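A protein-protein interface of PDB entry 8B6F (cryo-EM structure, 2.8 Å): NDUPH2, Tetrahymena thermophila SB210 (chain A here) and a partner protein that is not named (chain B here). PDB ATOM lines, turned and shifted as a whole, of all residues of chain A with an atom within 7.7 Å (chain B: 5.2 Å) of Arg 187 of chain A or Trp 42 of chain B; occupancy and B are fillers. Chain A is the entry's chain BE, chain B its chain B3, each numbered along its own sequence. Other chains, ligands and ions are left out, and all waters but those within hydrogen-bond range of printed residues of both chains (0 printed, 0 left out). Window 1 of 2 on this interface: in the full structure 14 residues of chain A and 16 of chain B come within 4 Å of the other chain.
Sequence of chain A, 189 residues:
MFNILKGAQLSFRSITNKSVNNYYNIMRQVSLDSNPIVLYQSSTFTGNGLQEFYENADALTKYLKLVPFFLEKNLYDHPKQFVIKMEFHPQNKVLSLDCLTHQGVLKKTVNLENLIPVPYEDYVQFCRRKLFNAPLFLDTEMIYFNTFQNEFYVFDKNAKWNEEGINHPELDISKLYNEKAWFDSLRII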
ATOM      1  N   ASP A 122     -21.554  12.676   0.732  1.00  0.00           N
ATOM      2  CA  ASP A 122     -22.910  12.138   0.728  1.00  0.00           C
ATOM      3  C   ASP A 122     -23.664  12.583  -0.516  1.00  0.00           C
ATOM      4  O   ASP A 122     -24.366  11.784  -1.145  1.00  0.00           O
ATOM      5  CB  ASP A 122     -23.657  12.582   1.985  1.00  0.00           C
ATOM      6  CG  ASP A 122     -23.235  11.809   3.213  1.00  0.00           C
ATOM      7  OD1 ASP A 122     -22.054  11.907   3.604  1.00  0.00           O
ATOM      8  OD2 ASP A 122     -24.088  11.104   3.791  1.00  0.00           O
ATOM      9  N   PHE A 126     -24.947   9.799  -3.242  1.00  0.00           N
ATOM     10  CA  PHE A 126     -26.374   9.565  -3.417  1.00  0.00           C
ATOM     11  C   PHE A 126     -26.663   8.987  -4.797  1.00  0.00           C
ATOM     12  O   PHE A 126     -27.453   8.046  -4.932  1.00  0.00           O
ATOM     13  CB  PHE A 126     -27.150  10.864  -3.206  1.00  0.00           C
ATOM     14  CG  PHE A 126     -28.638  10.685  -3.205  1.00  0.00           C
ATOM     15  CD1 PHE A 126     -29.311  10.396  -2.030  1.00  0.00           C
ATOM     16  CD2 PHE A 126     -29.367  10.816  -4.375  1.00  0.00           C
ATOM     17  CE1 PHE A 126     -30.679  10.234  -2.023  1.00  0.00           C
ATOM     18  CE2 PHE A 126     -30.736  10.656  -4.372  1.00  0.00           C
ATOM     19  CZ  PHE A 126     -31.393  10.365  -3.196  1.00  0.00           C
ATOM     20  N   PHE A 183     -28.440  13.152  11.608  1.00  0.00           N
ATOM     21  CA  PHE A 183     -27.396  12.137  11.545  1.00  0.00           C
ATOM     22  C   PHE A 183     -27.874  10.787  11.030  1.00  0.00           C
ATOM     23  O   PHE A 183     -27.073  10.045  10.455  1.00  0.00           O
ATOM     24  CB  PHE A 183     -26.770  11.940  12.929  1.00  0.00           C
ATOM     25  CG  PHE A 183     -25.961  13.112  13.400  1.00  0.00           C
ATOM     26  CD1 PHE A 183     -24.611  13.199  13.104  1.00  0.00           C
ATOM     27  CD2 PHE A 183     -26.548  14.124  14.140  1.00  0.00           C
ATOM     28  CE1 PHE A 183     -23.861  14.276  13.536  1.00  0.00           C
ATOM     29  CE2 PHE A 183     -25.803  15.204  14.576  1.00  0.00           C
ATOM     30  CZ  PHE A 183     -24.459  15.280  14.272  1.00  0.00           C
ATOM     31  N   ASP A 184     -29.149  10.449  11.211  1.00  0.00           N
ATOM     32  CA  ASP A 184     -29.642   9.115  10.899  1.00  0.00           C
ATOM     33  C   ASP A 184     -30.717   9.092   9.823  1.00  0.00           C
ATOM     34  O   ASP A 184     -31.162   8.002   9.445  1.00  0.00           O
ATOM     35  CB  ASP A 184     -30.190   8.448  12.168  1.00  0.00           C
ATOM     36  CG  ASP A 184     -29.168   8.396  13.286  1.00  0.00           C
ATOM     37  OD1 ASP A 184     -27.971   8.210  12.988  1.00  0.00           O
ATOM     38  OD2 ASP A 184     -29.560   8.546  14.463  1.00  0.00           O
ATOM     39  N   SER A 185     -31.151  10.247   9.319  1.00  0.00           N
ATOM     40  CA  SER A 185     -32.212  10.247   8.318  1.00  0.00           C
ATOM     41  C   SER A 185     -31.708   9.741   6.972  1.00  0.00           C
ATOM     42  O   SER A 185     -32.377   8.933   6.318  1.00  0.00           O
ATOM     43  CB  SER A 185     -32.795  11.652   8.174  1.00  0.00           C
ATOM     44  OG  SER A 185     -33.868  11.667   7.248  1.00  0.00           O
ATOM     45  N   LEU A 186     -30.537  10.201   6.542  1.00  0.00           N
ATOM     46  CA  LEU A 186     -29.981   9.859   5.234  1.00  0.00           C
ATOM     47  C   LEU A 186     -28.800   8.920   5.449  1.00  0.00           C
ATOM     48  O   LEU A 186     -27.712   9.355   5.837  1.00  0.00           O
ATOM     49  CB  LEU A 186     -29.567  11.117   4.475  1.00  0.00           C
ATOM     50  CG  LEU A 186     -29.046  10.909   3.053  1.00  0.00           C
ATOM     51  CD1 LEU A 186     -30.117  10.304   2.163  1.00  0.00           C
ATOM     52  CD2 LEU A 186     -28.550  12.220   2.470  1.00  0.00           C
ATOM     53  N   ARG A 187     -29.017   7.633   5.192  1.00  0.00           N
ATOM     54  CA  ARG A 187     -27.994   6.597   5.318  1.00  0.00           C
ATOM     55  C   ARG A 187     -27.811   5.991   3.930  1.00  0.00           C
ATOM     56  O   ARG A 187     -28.514   5.053   3.550  1.00  0.00           O
ATOM     57  CB  ARG A 187     -28.400   5.551   6.357  1.00  0.00           C
ATOM     58  CG  ARG A 187     -27.335   4.507   6.638  1.00  0.00           C
ATOM     59  CD  ARG A 187     -27.734   3.616   7.800  1.00  0.00           C
ATOM     60  NE  ARG A 187     -28.936   2.843   7.507  1.00  0.00           N
ATOM     61  CZ  ARG A 187     -28.943   1.625   6.981  1.00  0.00           C
ATOM     62  NH1 ARG A 187     -27.823   0.995   6.674  1.00  0.00           N
ATOM     63  NH2 ARG A 187     -30.109   1.023   6.759  1.00  0.00           N
ATOM     64  N   ILE A 188     -26.857   6.536   3.174  1.00  0.00           N
ATOM     65  CA  ILE A 188     -26.729   6.181   1.765  1.00  0.00           C
ATOM     66  C   ILE A 188     -26.312   4.723   1.608  1.00  0.00           C
ATOM     67  O   ILE A 188     -26.922   3.970   0.841  1.00  0.00           O
ATOM     68  CB  ILE A 188     -25.740   7.136   1.070  1.00  0.00           C
ATOM     69  CG1 ILE A 188     -26.377   8.518   0.916  1.00  0.00           C
ATOM     70  CG2 ILE A 188     -25.312   6.590  -0.291  1.00  0.00           C
ATOM     71  CD1 ILE A 188     -25.418   9.590   0.460  1.00  0.00           C
ATOM     72  N   ILE A 189     -25.283   4.301   2.338  1.00  0.00           N
ATOM     73  CA  ILE A 189     -24.686   2.971   2.175  1.00  0.00           C
ATOM     74  C   ILE A 189     -24.637   2.559   0.706  1.00  0.00           C
ATOM     75  O   ILE A 189     -24.709   1.374   0.381  1.00  0.00           O
ATOM     76  CB  ILE A 189     -25.432   1.899   3.002  1.00  0.00           C
ATOM     77  CG1 ILE A 189     -26.899   1.782   2.572  1.00  0.00           C
ATOM     78  CG2 ILE A 189     -25.316   2.214   4.482  1.00  0.00           C
ATOM     79  CD1 ILE A 189     -27.615   0.587   3.160  1.00  0.00           C
ATOM     80  OXT ILE A 189     -24.530   3.393  -0.192  1.00  0.00           O
ATOM     81  N   TYR B  35     -27.396   3.789  17.345  1.00  0.00           N
ATOM     82  CA  TYR B  35     -27.065   4.648  16.214  1.00  0.00           C
ATOM     83  C   TYR B  35     -25.720   5.329  16.420  1.00  0.00           C
ATOM     84  O   TYR B  35     -24.878   5.356  15.517  1.00  0.00           O
ATOM     85  CB  TYR B  35     -28.157   5.698  16.009  1.00  0.00           C
ATOM     86  CG  TYR B  35     -29.467   5.143  15.510  1.00  0.00           C
ATOM     87  CD1 TYR B  35     -29.717   5.024  14.150  1.00  0.00           C
ATOM     88  CD2 TYR B  35     -30.462   4.759  16.396  1.00  0.00           C
ATOM     89  CE1 TYR B  35     -30.913   4.526  13.687  1.00  0.00           C
ATOM     90  CE2 TYR B  35     -31.663   4.261  15.943  1.00  0.00           C
ATOM     91  CZ  TYR B  35     -31.883   4.147  14.587  1.00  0.00           C
ATOM     92  OH  TYR B  35     -33.080   3.649  14.130  1.00  0.00           O
ATOM     93  N   ASN B  38     -22.764   2.919  15.999  1.00  0.00           N
ATOM     94  CA  ASN B  38     -22.624   2.371  14.656  1.00  0.00           C
ATOM     95  C   ASN B  38     -22.481   3.431  13.568  1.00  0.00           C
ATOM     96  O   ASN B  38     -22.339   3.067  12.396  1.00  0.00           O
ATOM     97  CB  ASN B  38     -23.831   1.483  14.327  1.00  0.00           C
ATOM     98  CG  ASN B  38     -23.805   0.164  15.069  1.00  0.00           C
ATOM     99  OD1 ASN B  38     -23.101  -0.765  14.678  1.00  0.00           O
ATOM    100  ND2 ASN B  38     -24.591   0.067  16.134  1.00  0.00           N
ATOM    101  N   ARG B  39     -22.511   4.721  13.911  1.00  0.00           N
ATOM    102  CA  ARG B  39     -22.453   5.757  12.880  1.00  0.00           C
ATOM    103  C   ARG B  39     -21.265   5.571  11.945  1.00  0.00           C
ATOM    104  O   ARG B  39     -21.378   5.794  10.735  1.00  0.00           O
ATOM    105  CB  ARG B  39     -22.411   7.146  13.519  1.00  0.00           C
ATOM    106  CG  ARG B  39     -23.724   7.553  14.165  1.00  0.00           C
ATOM    107  CD  ARG B  39     -24.034   9.021  13.937  1.00  0.00           C
ATOM    108  NE  ARG B  39     -25.325   9.392  14.502  1.00  0.00           N
ATOM    109  CZ  ARG B  39     -25.508   9.866  15.726  1.00  0.00           C
ATOM    110  NH1 ARG B  39     -24.495  10.054  16.556  1.00  0.00           N
ATOM    111  NH2 ARG B  39     -26.740  10.159  16.131  1.00  0.00           N
ATOM    112  N   TRP B  40     -20.115   5.164  12.483  1.00  0.00           N
ATOM    113  CA  TRP B  40     -18.908   5.081  11.668  1.00  0.00           C
ATOM    114  C   TRP B  40     -19.052   4.106  10.507  1.00  0.00           C
ATOM    115  O   TRP B  40     -18.348   4.252   9.502  1.00  0.00           O
ATOM    116  CB  TRP B  40     -17.721   4.666  12.538  1.00  0.00           C
ATOM    117  CG  TRP B  40     -17.803   3.259  13.023  1.00  0.00           C
ATOM    118  CD1 TRP B  40     -18.360   2.826  14.186  1.00  0.00           C
ATOM    119  CD2 TRP B  40     -17.310   2.095  12.353  1.00  0.00           C
ATOM    120  NE1 TRP B  40     -18.245   1.461  14.284  1.00  0.00           N
ATOM    121  CE2 TRP B  40     -17.605   0.987  13.170  1.00  0.00           C
ATOM    122  CE3 TRP B  40     -16.650   1.882  11.138  1.00  0.00           C
ATOM    123  CZ2 TRP B  40     -17.260  -0.313  12.815  1.00  0.00           C
ATOM    124  CZ3 TRP B  40     -16.308   0.591  10.786  1.00  0.00           C
ATOM    125  CH2 TRP B  40     -16.615  -0.492  11.620  1.00  0.00           C
ATOM    126  N   ARG B  41     -19.946   3.121  10.616  1.00  0.00           N
ATOM    127  CA  ARG B  41     -20.001   2.060   9.615  1.00  0.00           C
ATOM    128  C   ARG B  41     -20.369   2.600   8.240  1.00  0.00           C
ATOM    129  O   ARG B  41     -19.799   2.180   7.228  1.00  0.00           O
ATOM    130  CB  ARG B  41     -20.996   0.986  10.047  1.00  0.00           C
ATOM    131  CG  ARG B  41     -20.552   0.201  11.262  1.00  0.00           C
ATOM    132  CD  ARG B  41     -21.485  -0.960  11.542  1.00  0.00           C
ATOM    133  NE  ARG B  41     -20.978  -1.795  12.623  1.00  0.00           N
ATOM    134  CZ  ARG B  41     -20.034  -2.714  12.478  1.00  0.00           C
ATOM    135  NH1 ARG B  41     -19.460  -2.936  11.309  1.00  0.00           N
ATOM    136  NH2 ARG B  41     -19.648  -3.420  13.535  1.00  0.00           N
ATOM    137  N   TRP B  42     -21.321   3.531   8.178  1.00  0.00           N
ATOM    138  CA  TRP B  42     -21.880   3.990   6.913  1.00  0.00           C
ATOM    139  C   TRP B  42     -21.244   5.288   6.430  1.00  0.00           C
ATOM    140  O   TRP B  42     -21.912   6.106   5.791  1.00  0.00           O
ATOM    141  CB  TRP B  42     -23.393   4.150   7.044  1.00  0.00           C
ATOM    142  CG  TRP B  42     -24.005   3.073   7.876  1.00  0.00           C
ATOM    143  CD1 TRP B  42     -24.196   1.768   7.522  1.00  0.00           C
ATOM    144  CD2 TRP B  42     -24.497   3.205   9.211  1.00  0.00           C
ATOM    145  NE1 TRP B  42     -24.782   1.081   8.557  1.00  0.00           N
ATOM    146  CE2 TRP B  42     -24.976   1.941   9.606  1.00  0.00           C
ATOM    147  CE3 TRP B  42     -24.580   4.270  10.110  1.00  0.00           C
ATOM    148  CZ2 TRP B  42     -25.531   1.716  10.860  1.00  0.00           C
ATOM    149  CZ3 TRP B  42     -25.132   4.045  11.355  1.00  0.00           C
ATOM    150  CH2 TRP B  42     -25.601   2.778  11.720  1.00  0.00           C
ATOM    151  N   ASN B  43     -19.963   5.492   6.722  1.00  0.00           N
ATOM    152  CA  ASN B  43     -19.268   6.671   6.227  1.00  0.00           C
ATOM    153  C   ASN B  43     -19.214   6.640   4.706  1.00  0.00           C
ATOM    154  O   ASN B  43     -18.805   5.643   4.106  1.00  0.00           O
ATOM    155  CB  ASN B  43     -17.856   6.725   6.811  1.00  0.00           C
ATOM    156  CG  ASN B  43     -17.138   8.019   6.489  1.00  0.00           C
ATOM    157  OD1 ASN B  43     -17.475   8.710   5.530  1.00  0.00           O
ATOM    158  ND2 ASN B  43     -16.134   8.350   7.291  1.00  0.00           N
ATOM    159  N   THR B  44     -19.630   7.742   4.080  1.00  0.00           N
ATOM    160  CA  THR B  44     -19.604   7.821   2.625  1.00  0.00           C
ATOM    161  C   THR B  44     -18.194   8.027   2.089  1.00  0.00           C
ATOM    162  O   THR B  44     -17.907   7.643   0.951  1.00  0.00           O
ATOM    163  CB  THR B  44     -20.520   8.946   2.142  1.00  0.00           C
ATOM    164  OG1 THR B  44     -20.241  10.144   2.876  1.00  0.00           O
ATOM    165  CG2 THR B  44     -21.978   8.560   2.329  1.00  0.00           C
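Of the printed residues of chain B, Phe 183 of chain A touches Arg 39.
Leu 186 of chain A touches none of the printed residues of chain B.
Arg 187 of chain A touches just one residue of chain B: Trp 42 (3.6 Å).
Of chain A, only Arg 187 (3.6 Å) and Ile 189 (3.3 Å) come within 4 Å of Trp 42 of chain B.
Printed residues of chain A within 4 Å of Thr 44 of chain B: Asp 122.
The nearest printed residue of chain B that does not touch Arg 187 of chain A is Thr 44 of chain B (6.6 Å).
The nearest printed residue of chain B that does not touch Phe 183 of chain A is Trp 42 of chain B (6.3 Å).
Hydrophobic or aromatic side chains of chain B that line the printed part of chain A: Tyr 35 and Trp 42.
Printed residues of chain A that touch a printed residue of chain B: Asp 122, Phe 183, Asp 184, Arg 187 and Ile 189.
Hydrophobic or aromatic side chains of chain A within 4 Å of the printed part of chain B: Phe 183 and Ile 189.
Among the printed residues, 6 pairs touch across the chains.
Among the printed residues, Asp or Glu carboxylates within 4 Å of a Lys or Arg side-chain nitrogen of the other chain: Asp 184 of chain A with Arg 39 of chain B.
Arg 39 of chain B touches Phe 183 of chain A (NE to CB, 3.3 Å).
CD1 of Tyr 35 of chain B touches CG of Asp 184 of chain A (3.5 Å).
Arg 187 of chain A touches Trp 42 of chain B.
Ile 189 of chain A touches Trp 42 of chain B.
The guanidinium group of Arg 39 of chain B is in salt-bridge range of the side-chain carboxylate of Asp 184 of chain A (3.3 Å).
The side-chain carboxylate (OD1) of Asp 122 of chain A lies within hydrogen-bond range of the side-chain hydroxyl (OG1) of Thr 44 of chain B, at 2.6 Å.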
